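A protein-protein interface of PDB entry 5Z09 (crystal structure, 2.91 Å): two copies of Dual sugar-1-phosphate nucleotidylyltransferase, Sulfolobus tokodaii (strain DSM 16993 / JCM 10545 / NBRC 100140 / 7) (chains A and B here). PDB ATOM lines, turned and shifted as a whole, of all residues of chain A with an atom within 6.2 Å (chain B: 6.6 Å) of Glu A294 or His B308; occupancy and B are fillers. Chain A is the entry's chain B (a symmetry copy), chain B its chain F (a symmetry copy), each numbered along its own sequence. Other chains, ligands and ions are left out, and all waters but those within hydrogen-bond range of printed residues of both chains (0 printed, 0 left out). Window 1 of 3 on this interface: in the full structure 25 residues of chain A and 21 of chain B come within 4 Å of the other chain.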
ATOM      1  N   SER A 275     -24.489  -5.791 -17.664  1.00  0.00           N
ATOM      2  CA  SER A 275     -25.052  -4.897 -16.660  1.00  0.00           C
ATOM      3  C   SER A 275     -24.182  -4.818 -15.401  1.00  0.00           C
ATOM      4  O   SER A 275     -23.210  -5.551 -15.257  1.00  0.00           O
ATOM      5  CB  SER A 275     -26.436  -5.376 -16.252  1.00  0.00           C
ATOM      6  OG  SER A 275     -27.319  -5.380 -17.357  1.00  0.00           O
ATOM      7  N   TYR A 276     -24.478  -3.852 -14.536  1.00  0.00           N
ATOM      8  CA  TYR A 276     -23.648  -3.583 -13.357  1.00  0.00           C
ATOM      9  C   TYR A 276     -24.553  -3.207 -12.195  1.00  0.00           C
ATOM     10  O   TYR A 276     -25.047  -2.078 -12.129  1.00  0.00           O
ATOM     11  CB  TYR A 276     -22.654  -2.446 -13.649  1.00  0.00           C
ATOM     12  CG  TYR A 276     -21.717  -2.070 -12.510  1.00  0.00           C
ATOM     13  CD1 TYR A 276     -21.425  -2.958 -11.491  1.00  0.00           C
ATOM     14  CD2 TYR A 276     -21.040  -0.849 -12.520  1.00  0.00           C
ATOM     15  CE1 TYR A 276     -20.542  -2.616 -10.478  1.00  0.00           C
ATOM     16  CE2 TYR A 276     -20.146  -0.503 -11.520  1.00  0.00           C
ATOM     17  CZ  TYR A 276     -19.891  -1.393 -10.506  1.00  0.00           C
ATOM     18  OH  TYR A 276     -18.986  -1.068  -9.517  1.00  0.00           O
ATOM     19  N   LEU A 277     -24.838  -4.171 -11.332  1.00  0.00           N
ATOM     20  CA  LEU A 277     -25.621  -3.898 -10.131  1.00  0.00           C
ATOM     21  C   LEU A 277     -24.760  -3.663  -8.889  1.00  0.00           C
ATOM     22  O   LEU A 277     -24.003  -4.541  -8.473  1.00  0.00           O
ATOM     23  CB  LEU A 277     -26.574  -5.050  -9.871  1.00  0.00           C
ATOM     24  CG  LEU A 277     -27.308  -5.540 -11.119  1.00  0.00           C
ATOM     25  CD1 LEU A 277     -28.266  -6.686 -10.787  1.00  0.00           C
ATOM     26  CD2 LEU A 277     -28.046  -4.386 -11.771  1.00  0.00           C
ATOM     27  N   ARG A 278     -24.882  -2.478  -8.300  1.00  0.00           N
ATOM     28  CA  ARG A 278     -24.067  -2.087  -7.145  1.00  0.00           C
ATOM     29  C   ARG A 278     -24.858  -2.158  -5.846  1.00  0.00           C
ATOM     30  O   ARG A 278     -26.056  -2.451  -5.854  1.00  0.00           O
ATOM     31  CB  ARG A 278     -23.505  -0.674  -7.352  1.00  0.00           C
ATOM     32  CG  ARG A 278     -22.400  -0.634  -8.401  1.00  0.00           C
ATOM     33  CD  ARG A 278     -22.080   0.797  -8.779  1.00  0.00           C
ATOM     34  NE  ARG A 278     -21.768   1.546  -7.578  1.00  0.00           N
ATOM     35  CZ  ARG A 278     -21.791   2.866  -7.474  1.00  0.00           C
ATOM     36  NH1 ARG A 278     -22.140   3.624  -8.503  1.00  0.00           N
ATOM     37  NH2 ARG A 278     -21.475   3.428  -6.312  1.00  0.00           N
ATOM     38  N   ILE A 289     -32.960  -5.342 -16.720  1.00  0.00           N
ATOM     39  CA  ILE A 289     -31.791  -4.475 -16.733  1.00  0.00           C
ATOM     40  C   ILE A 289     -30.880  -4.927 -17.857  1.00  0.00           C
ATOM     41  O   ILE A 289     -30.579  -6.111 -17.974  1.00  0.00           O
ATOM     42  CB  ILE A 289     -31.005  -4.545 -15.399  1.00  0.00           C
ATOM     43  CG1 ILE A 289     -31.919  -4.230 -14.215  1.00  0.00           C
ATOM     44  CG2 ILE A 289     -29.811  -3.582 -15.435  1.00  0.00           C
ATOM     45  CD1 ILE A 289     -32.423  -2.798 -14.191  1.00  0.00           C
ATOM     46  N   GLY A 290     -30.354  -3.975 -18.605  1.00  0.00           N
ATOM     47  CA  GLY A 290     -29.774  -4.280 -19.894  1.00  0.00           C
ATOM     48  C   GLY A 290     -28.319  -3.882 -20.027  1.00  0.00           C
ATOM     49  O   GLY A 290     -27.672  -3.498 -19.062  1.00  0.00           O
ATOM     50  N   SER A 292     -24.898  -2.020 -20.619  1.00  0.00           N
ATOM     51  CA  SER A 292     -24.408  -0.724 -20.216  1.00  0.00           C
ATOM     52  C   SER A 292     -25.427   0.007 -19.347  1.00  0.00           C
ATOM     53  O   SER A 292     -25.545   1.226 -19.409  1.00  0.00           O
ATOM     54  CB  SER A 292     -24.018   0.117 -21.440  1.00  0.00           C
ATOM     55  OG  SER A 292     -23.093  -0.588 -22.234  1.00  0.00           O
ATOM     56  N   VAL A 293     -26.093  -0.739 -18.477  1.00  0.00           N
ATOM     57  CA  VAL A 293     -26.924  -0.135 -17.456  1.00  0.00           C
ATOM     58  C   VAL A 293     -26.344  -0.397 -16.073  1.00  0.00           C
ATOM     59  O   VAL A 293     -25.917  -1.505 -15.771  1.00  0.00           O
ATOM     60  CB  VAL A 293     -28.347  -0.699 -17.517  1.00  0.00           C
ATOM     61  CG1 VAL A 293     -29.216  -0.110 -16.414  1.00  0.00           C
ATOM     62  CG2 VAL A 293     -28.948  -0.434 -18.894  1.00  0.00           C
ATOM     63  N   GLU A 294     -26.339   0.635 -15.235  1.00  0.00           N
ATOM     64  CA  GLU A 294     -25.792   0.552 -13.881  1.00  0.00           C
ATOM     65  C   GLU A 294     -26.860   0.987 -12.889  1.00  0.00           C
ATOM     66  O   GLU A 294     -27.436   2.064 -13.008  1.00  0.00           O
ATOM     67  CB  GLU A 294     -24.551   1.454 -13.771  1.00  0.00           C
ATOM     68  CG  GLU A 294     -23.915   1.523 -12.388  1.00  0.00           C
ATOM     69  CD  GLU A 294     -22.663   2.399 -12.340  1.00  0.00           C
ATOM     70  OE1 GLU A 294     -22.018   2.641 -13.379  1.00  0.00           O
ATOM     71  OE2 GLU A 294     -22.341   2.890 -11.255  1.00  0.00           O
ATOM     72  N   VAL A 295     -27.138   0.144 -11.915  1.00  0.00           N
ATOM     73  CA  VAL A 295     -28.055   0.502 -10.836  1.00  0.00           C
ATOM     74  C   VAL A 295     -27.289   0.611  -9.522  1.00  0.00           C
ATOM     75  O   VAL A 295     -26.315  -0.108  -9.302  1.00  0.00           O
ATOM     76  CB  VAL A 295     -29.159  -0.556 -10.689  1.00  0.00           C
ATOM     77  CG1 VAL A 295     -30.172  -0.126  -9.649  1.00  0.00           C
ATOM     78  CG2 VAL A 295     -29.838  -0.783 -12.022  1.00  0.00           C
ATOM     79  N   LYS A 296     -27.753   1.474  -8.631  1.00  0.00           N
ATOM     80  CA  LYS A 296     -27.129   1.635  -7.306  1.00  0.00           C
ATOM     81  C   LYS A 296     -28.134   2.145  -6.286  1.00  0.00           C
ATOM     82  O   LYS A 296     -28.818   3.132  -6.533  1.00  0.00           O
ATOM     83  CB  LYS A 296     -25.946   2.614  -7.366  1.00  0.00           C
ATOM     84  CG  LYS A 296     -25.082   2.593  -6.121  1.00  0.00           C
ATOM     85  CD  LYS A 296     -24.512   3.966  -5.797  1.00  0.00           C
ATOM     86  CE  LYS A 296     -25.485   4.841  -5.041  1.00  0.00           C
ATOM     87  NZ  LYS A 296     -24.829   6.033  -4.433  1.00  0.00           N
ATOM     88  N   SER A 310     -27.900   3.479 -19.209  1.00  0.00           N
ATOM     89  CA  SER A 310     -28.504   4.288 -18.166  1.00  0.00           C
ATOM     90  C   SER A 310     -27.830   4.068 -16.839  1.00  0.00           C
ATOM     91  O   SER A 310     -27.269   3.006 -16.583  1.00  0.00           O
ATOM     92  CB  SER A 310     -29.978   3.940 -17.996  1.00  0.00           C
ATOM     93  OG  SER A 310     -30.671   4.098 -19.218  1.00  0.00           O
ATOM     94  N   TYR A 311     -27.898   5.083 -15.990  1.00  0.00           N
ATOM     95  CA  TYR A 311     -27.449   4.972 -14.614  1.00  0.00           C
ATOM     96  C   TYR A 311     -28.585   5.406 -13.714  1.00  0.00           C
ATOM     97  O   TYR A 311     -29.076   6.532 -13.816  1.00  0.00           O
ATOM     98  CB  TYR A 311     -26.212   5.847 -14.364  1.00  0.00           C
ATOM     99  CG  TYR A 311     -25.815   5.937 -12.909  1.00  0.00           C
ATOM    100  CD1 TYR A 311     -25.492   4.798 -12.189  1.00  0.00           C
ATOM    101  CD2 TYR A 311     -25.776   7.153 -12.257  1.00  0.00           C
ATOM    102  CE1 TYR A 311     -25.152   4.872 -10.853  1.00  0.00           C
ATOM    103  CE2 TYR A 311     -25.411   7.244 -10.928  1.00  0.00           C
ATOM    104  CZ  TYR A 311     -25.100   6.100 -10.231  1.00  0.00           C
ATOM    105  OH  TYR A 311     -24.749   6.184  -8.903  1.00  0.00           O
ATOM    106  N   VAL A 312     -28.998   4.501 -12.842  1.00  0.00           N
ATOM    107  CA  VAL A 312     -29.983   4.805 -11.838  1.00  0.00           C
ATOM    108  C   VAL A 312     -29.287   4.714 -10.481  1.00  0.00           C
ATOM    109  O   VAL A 312     -28.913   3.634 -10.049  1.00  0.00           O
ATOM    110  CB  VAL A 312     -31.175   3.817 -11.915  1.00  0.00           C
ATOM    111  CG1 VAL A 312     -32.222   4.123 -10.860  1.00  0.00           C
ATOM    112  CG2 VAL A 312     -31.807   3.866 -13.288  1.00  0.00           C
ATOM    113  N   GLY A 313     -29.234   5.831  -9.763  1.00  0.00           N
ATOM    114  CA  GLY A 313     -28.656   5.857  -8.417  1.00  0.00           C
ATOM    115  C   GLY A 313     -29.609   6.447  -7.395  1.00  0.00           C
ATOM    116  O   GLY A 313     -30.275   7.444  -7.657  1.00  0.00           O
ATOM    117  N   LYS B 288     -10.451   7.124 -10.665  1.00  0.00           N
ATOM    118  CA  LYS B 288     -11.614   6.229 -10.788  1.00  0.00           C
ATOM    119  C   LYS B 288     -12.088   6.205 -12.234  1.00  0.00           C
ATOM    120  O   LYS B 288     -12.452   7.239 -12.789  1.00  0.00           O
ATOM    121  CB  LYS B 288     -12.755   6.734  -9.900  1.00  0.00           C
ATOM    122  CG  LYS B 288     -14.073   5.991 -10.059  1.00  0.00           C
ATOM    123  CD  LYS B 288     -14.033   4.649  -9.349  1.00  0.00           C
ATOM    124  CE  LYS B 288     -15.034   3.672  -9.914  1.00  0.00           C
ATOM    125  NZ  LYS B 288     -16.189   3.516  -9.005  1.00  0.00           N
ATOM    126  N   ILE B 289     -12.014   5.041 -12.863  1.00  0.00           N
ATOM    127  CA  ILE B 289     -12.656   4.835 -14.156  1.00  0.00           C
ATOM    128  C   ILE B 289     -13.665   3.714 -14.003  1.00  0.00           C
ATOM    129  O   ILE B 289     -13.353   2.644 -13.469  1.00  0.00           O
ATOM    130  CB  ILE B 289     -11.650   4.438 -15.242  1.00  0.00           C
ATOM    131  CG1 ILE B 289     -10.523   5.474 -15.334  1.00  0.00           C
ATOM    132  CG2 ILE B 289     -12.358   4.276 -16.579  1.00  0.00           C
ATOM    133  CD1 ILE B 289     -10.968   6.834 -15.818  1.00  0.00           C
ATOM    134  N   GLY B 290     -14.868   3.950 -14.509  1.00  0.00           N
ATOM    135  CA  GLY B 290     -16.007   3.117 -14.164  1.00  0.00           C
ATOM    136  C   GLY B 290     -16.654   2.407 -15.346  1.00  0.00           C
ATOM    137  O   GLY B 290     -16.091   2.329 -16.443  1.00  0.00           O
ATOM    138  N   ALA B 291     -17.828   1.844 -15.088  1.00  0.00           N
ATOM    139  CA  ALA B 291     -18.525   1.018 -16.055  1.00  0.00           C
ATOM    140  C   ALA B 291     -18.927   1.829 -17.278  1.00  0.00           C
ATOM    141  O   ALA B 291     -19.382   2.964 -17.159  1.00  0.00           O
ATOM    142  CB  ALA B 291     -19.753   0.371 -15.422  1.00  0.00           C
ATOM    143  N   SER B 292     -18.759   1.214 -18.448  1.00  0.00           N
ATOM    144  CA  SER B 292     -19.042   1.846 -19.711  1.00  0.00           C
ATOM    145  C   SER B 292     -18.328   3.193 -19.851  1.00  0.00           C
ATOM    146  O   SER B 292     -18.869   4.149 -20.421  1.00  0.00           O
ATOM    147  CB  SER B 292     -20.547   1.998 -19.891  1.00  0.00           C
ATOM    148  OG  SER B 292     -21.175   0.751 -19.722  1.00  0.00           O
ATOM    149  N   VAL B 293     -17.082   3.239 -19.402  1.00  0.00           N
ATOM    150  CA  VAL B 293     -16.246   4.414 -19.626  1.00  0.00           C
ATOM    151  C   VAL B 293     -15.061   4.044 -20.499  1.00  0.00           C
ATOM    152  O   VAL B 293     -14.434   3.003 -20.291  1.00  0.00           O
ATOM    153  CB  VAL B 293     -15.728   4.988 -18.293  1.00  0.00           C
ATOM    154  CG1 VAL B 293     -14.801   6.177 -18.539  1.00  0.00           C
ATOM    155  CG2 VAL B 293     -16.902   5.383 -17.406  1.00  0.00           C
ATOM    156  N   ILE B 306     -13.997   9.427 -13.447  1.00  0.00           N
ATOM    157  CA  ILE B 306     -14.907   9.307 -14.585  1.00  0.00           C
ATOM    158  C   ILE B 306     -15.731   8.025 -14.398  1.00  0.00           C
ATOM    159  O   ILE B 306     -15.322   6.957 -14.842  1.00  0.00           O
ATOM    160  CB  ILE B 306     -14.129   9.196 -15.915  1.00  0.00           C
ATOM    161  CG1 ILE B 306     -12.903  10.121 -15.941  1.00  0.00           C
ATOM    162  CG2 ILE B 306     -15.040   9.486 -17.091  1.00  0.00           C
ATOM    163  CD1 ILE B 306     -13.238  11.591 -16.044  1.00  0.00           C
ATOM    164  N   PRO B 307     -16.805   8.096 -13.600  1.00  0.00           N
ATOM    165  CA  PRO B 307     -17.415   6.860 -13.076  1.00  0.00           C
ATOM    166  C   PRO B 307     -18.446   6.140 -13.960  1.00  0.00           C
ATOM    167  O   PRO B 307     -18.683   4.961 -13.744  1.00  0.00           O
ATOM    168  CB  PRO B 307     -18.100   7.329 -11.784  1.00  0.00           C
ATOM    169  CG  PRO B 307     -18.287   8.793 -11.955  1.00  0.00           C
ATOM    170  CD  PRO B 307     -17.089   9.250 -12.730  1.00  0.00           C
ATOM    171  N   HIS B 308     -19.117   6.847 -14.878  1.00  0.00           N
ATOM    172  CA  HIS B 308     -20.144   6.209 -15.725  1.00  0.00           C
ATOM    173  C   HIS B 308     -20.272   6.771 -17.139  1.00  0.00           C
ATOM    174  O   HIS B 308     -20.361   7.981 -17.336  1.00  0.00           O
ATOM    175  CB  HIS B 308     -21.517   6.304 -15.086  1.00  0.00           C
ATOM    176  CG  HIS B 308     -21.494   6.458 -13.608  1.00  0.00           C
ATOM    177  ND1 HIS B 308     -21.625   5.389 -12.752  1.00  0.00           N
ATOM    178  CD2 HIS B 308     -21.525   7.571 -12.841  1.00  0.00           C
ATOM    179  CE1 HIS B 308     -21.700   5.839 -11.515  1.00  0.00           C
ATOM    180  NE2 HIS B 308     -21.610   7.156 -11.541  1.00  0.00           N
ATOM    181  N   LEU B 309     -20.419   5.862 -18.097  1.00  0.00           N
ATOM    182  CA  LEU B 309     -21.009   6.173 -19.380  1.00  0.00           C
ATOM    183  C   LEU B 309     -20.369   7.416 -20.008  1.00  0.00           C
ATOM    184  O   LEU B 309     -21.060   8.359 -20.372  1.00  0.00           O
ATOM    185  CB  LEU B 309     -22.510   6.365 -19.205  1.00  0.00           C
ATOM    186  CG  LEU B 309     -23.284   5.077 -18.887  1.00  0.00           C
ATOM    187  CD1 LEU B 309     -24.528   5.340 -18.033  1.00  0.00           C
ATOM    188  CD2 LEU B 309     -23.670   4.354 -20.174  1.00  0.00           C
ATOM    189  N   SER B 310     -19.056   7.386 -20.201  1.00  0.00           N
ATOM    190  CA  SER B 310     -18.334   8.536 -20.734  1.00  0.00           C
ATOM    191  C   SER B 310     -17.239   8.103 -21.679  1.00  0.00           C
ATOM    192  O   SER B 310     -16.695   7.004 -21.563  1.00  0.00           O
ATOM    193  CB  SER B 310     -17.692   9.340 -19.601  1.00  0.00           C
ATOM    194  OG  SER B 310     -18.661   9.761 -18.660  1.00  0.00           O
ATOM    195  N   TYR B 311     -16.877   9.004 -22.582  1.00  0.00           N
ATOM    196  CA  TYR B 311     -15.726   8.807 -23.460  1.00  0.00           C
ATOM    197  C   TYR B 311     -14.838  10.036 -23.371  1.00  0.00           C
ATOM    198  O   TYR B 311     -15.281  11.163 -23.633  1.00  0.00           O
ATOM    199  CB  TYR B 311     -16.160   8.595 -24.923  1.00  0.00           C
ATOM    200  CG  TYR B 311     -15.003   8.593 -25.908  1.00  0.00           C
ATOM    201  CD1 TYR B 311     -13.986   7.668 -25.807  1.00  0.00           C
ATOM    202  CD2 TYR B 311     -14.914   9.551 -26.905  1.00  0.00           C
ATOM    203  CE1 TYR B 311     -12.914   7.686 -26.685  1.00  0.00           C
ATOM    204  CE2 TYR B 311     -13.845   9.578 -27.788  1.00  0.00           C
ATOM    205  CZ  TYR B 311     -12.840   8.654 -27.665  1.00  0.00           C
ATOM    206  OH  TYR B 311     -11.799   8.648 -28.581  1.00  0.00           O
ATOM    207  N   PHE B 323     -16.424  13.965 -13.562  1.00  0.00           N
ATOM    208  CA  PHE B 323     -17.361  13.915 -14.683  1.00  0.00           C
ATOM    209  C   PHE B 323     -18.663  13.214 -14.237  1.00  0.00           C
ATOM    210  O   PHE B 323     -18.649  12.070 -13.779  1.00  0.00           O
ATOM    211  CB  PHE B 323     -16.738  13.175 -15.874  1.00  0.00           C
ATOM    212  CG  PHE B 323     -15.919  14.046 -16.786  1.00  0.00           C
ATOM    213  CD1 PHE B 323     -15.390  15.251 -16.351  1.00  0.00           C
ATOM    214  CD2 PHE B 323     -15.667  13.645 -18.096  1.00  0.00           C
ATOM    215  CE1 PHE B 323     -14.643  16.051 -17.205  1.00  0.00           C
ATOM    216  CE2 PHE B 323     -14.908  14.431 -18.947  1.00  0.00           C
ATOM    217  CZ  PHE B 323     -14.401  15.641 -18.504  1.00  0.00           C
ATOM    218  N   GLY B 324     -19.783  13.909 -14.390  1.00  0.00           N
ATOM    219  CA  GLY B 324     -21.090  13.298 -14.208  1.00  0.00           C
ATOM    220  C   GLY B 324     -21.354  12.205 -15.232  1.00  0.00           C
ATOM    221  O   GLY B 324     -20.810  12.230 -16.342  1.00  0.00           O
ATOM    222  N   ALA B 325     -22.215  11.253 -14.880  1.00  0.00           N
ATOM    223  CA  ALA B 325     -22.604  10.211 -15.828  1.00  0.00           C
ATOM    224  C   ALA B 325     -22.982  10.835 -17.163  1.00  0.00           C
ATOM    225  O   ALA B 325     -23.692  11.831 -17.207  1.00  0.00           O
ATOM    226  CB  ALA B 325     -23.764   9.397 -15.282  1.00  0.00           C
ATOM    227  N   GLY B 326     -22.499  10.254 -18.255  1.00  0.00           N
ATOM    228  CA  GLY B 326     -22.901  10.690 -19.586  1.00  0.00           C
ATOM    229  C   GLY B 326     -22.118  11.870 -20.143  1.00  0.00           C
ATOM    230  O   GLY B 326     -22.428  12.357 -21.225  1.00  0.00           O
ATOM    231  N   THR B 327     -21.102  12.326 -19.420  1.00  0.00           N
ATOM    232  CA  THR B 327     -20.269  13.434 -19.894  1.00  0.00           C
ATOM    233  C   THR B 327     -19.420  12.951 -21.061  1.00  0.00           C
ATOM    234  O   THR B 327     -18.732  11.949 -20.943  1.00  0.00           O
ATOM    235  CB  THR B 327     -19.318  13.957 -18.787  1.00  0.00           C
ATOM    236  OG1 THR B 327     -20.077  14.405 -17.658  1.00  0.00           O
ATOM    237  CG2 THR B 327     -18.483  15.120 -19.304  1.00  0.00           C
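The side-chain hydroxyl (OG) of Ser A292 sits close to the side-chain hydroxyl (OG) of Ser B292, 3.4 Å away.
ND1 of His B308 sits at hydrogen-bond distance from OE1 of Glu A294 (2.8 Å).
N of Gly B326 is in hydrogen-bond range of O of His B308, 3.3 Å away.
OE2 of Glu A294 lies within salt-bridge range of NH1 of Arg A278, 2.9 Å away.
The backbone NH (N) of Glu A294 lies within hydrogen-bond range of the backbone carbonyl oxygen (O) of Ser A310 (2.9 Å).
The backbone NH (N) of Ser A310 lies within hydrogen-bond range of the backbone carbonyl oxygen (O) of Ser A292 (3.3 Å).
The backbone carbonyl oxygen (O) of Leu B309 sits close to the backbone NH (N) of Gly B326.
The backbone carbonyl oxygen of His B308 sits at hydrogen-bond distance from the side-chain hydroxyl of Ser B310.
Among the printed residues, merely in contact across the chains: Tyr A276 with Ala B291 (3.4 Å), Tyr A311 with His B308 (3.6 Å), Ser A292 with Leu B309 (3.7 Å), Ser A310 with Leu B309 (3.7 Å), Arg A278 with His B308 (3.8 Å), Glu A294 with Ala B291 (3.8 Å) and Tyr A311 with Leu B309 (3.9 Å).
Of the printed residues of chain B, Tyr A276 touches Ala B291.
Of chain B, only Ala B291 and His B308 come within 4 Å of Glu A294.
Of the printed residues of chain B, Tyr A311 touches His B308 (3.6 Å) and Leu B309 (3.9 Å).
Gly B290 touches none of the printed residues of chain A.
Of the printed residues of chain A, His B308 touches Arg A278, Glu A294 and Tyr A311.
Printed residues of chain A within 4 Å of Leu B309: Ser A292, Ser A310 and Tyr A311.
The nearest residue of chain B that does not touch Glu A294 is Pro B307 (4.1 Å).
The nearest printed residue of chain A that does not touch His B308 is Tyr A276 (6.2 Å).
Printed residues of chain A that touch a printed residue of chain B: Tyr A276, Arg A278, Ser A292, Glu A294, Ser A310 and Tyr A311.
Hydrophobic or aromatic side chains of chain A within 4 Å of the printed part of chain B: Tyr A276 and Tyr A311.
Along chain A the printed residues that touch a printed residue of chain B span positions 276 to 311.
Hydrophobic or aromatic side chains of chain B within 4 Å of the printed part of chain A: Ala B291, His B308 and Leu B309.
Among the printed residues, no Asp or Glu carboxylate lies within 4 Å of a Lys or Arg side-chain nitrogen of the other chain.
Ser B292 touches its own counterpart, Ser A292.
6 positions are printed for both chains.
Of the 9 pairs that touch across the chains among the printed residues, 1 has its exchanged pair printed and touching as well.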
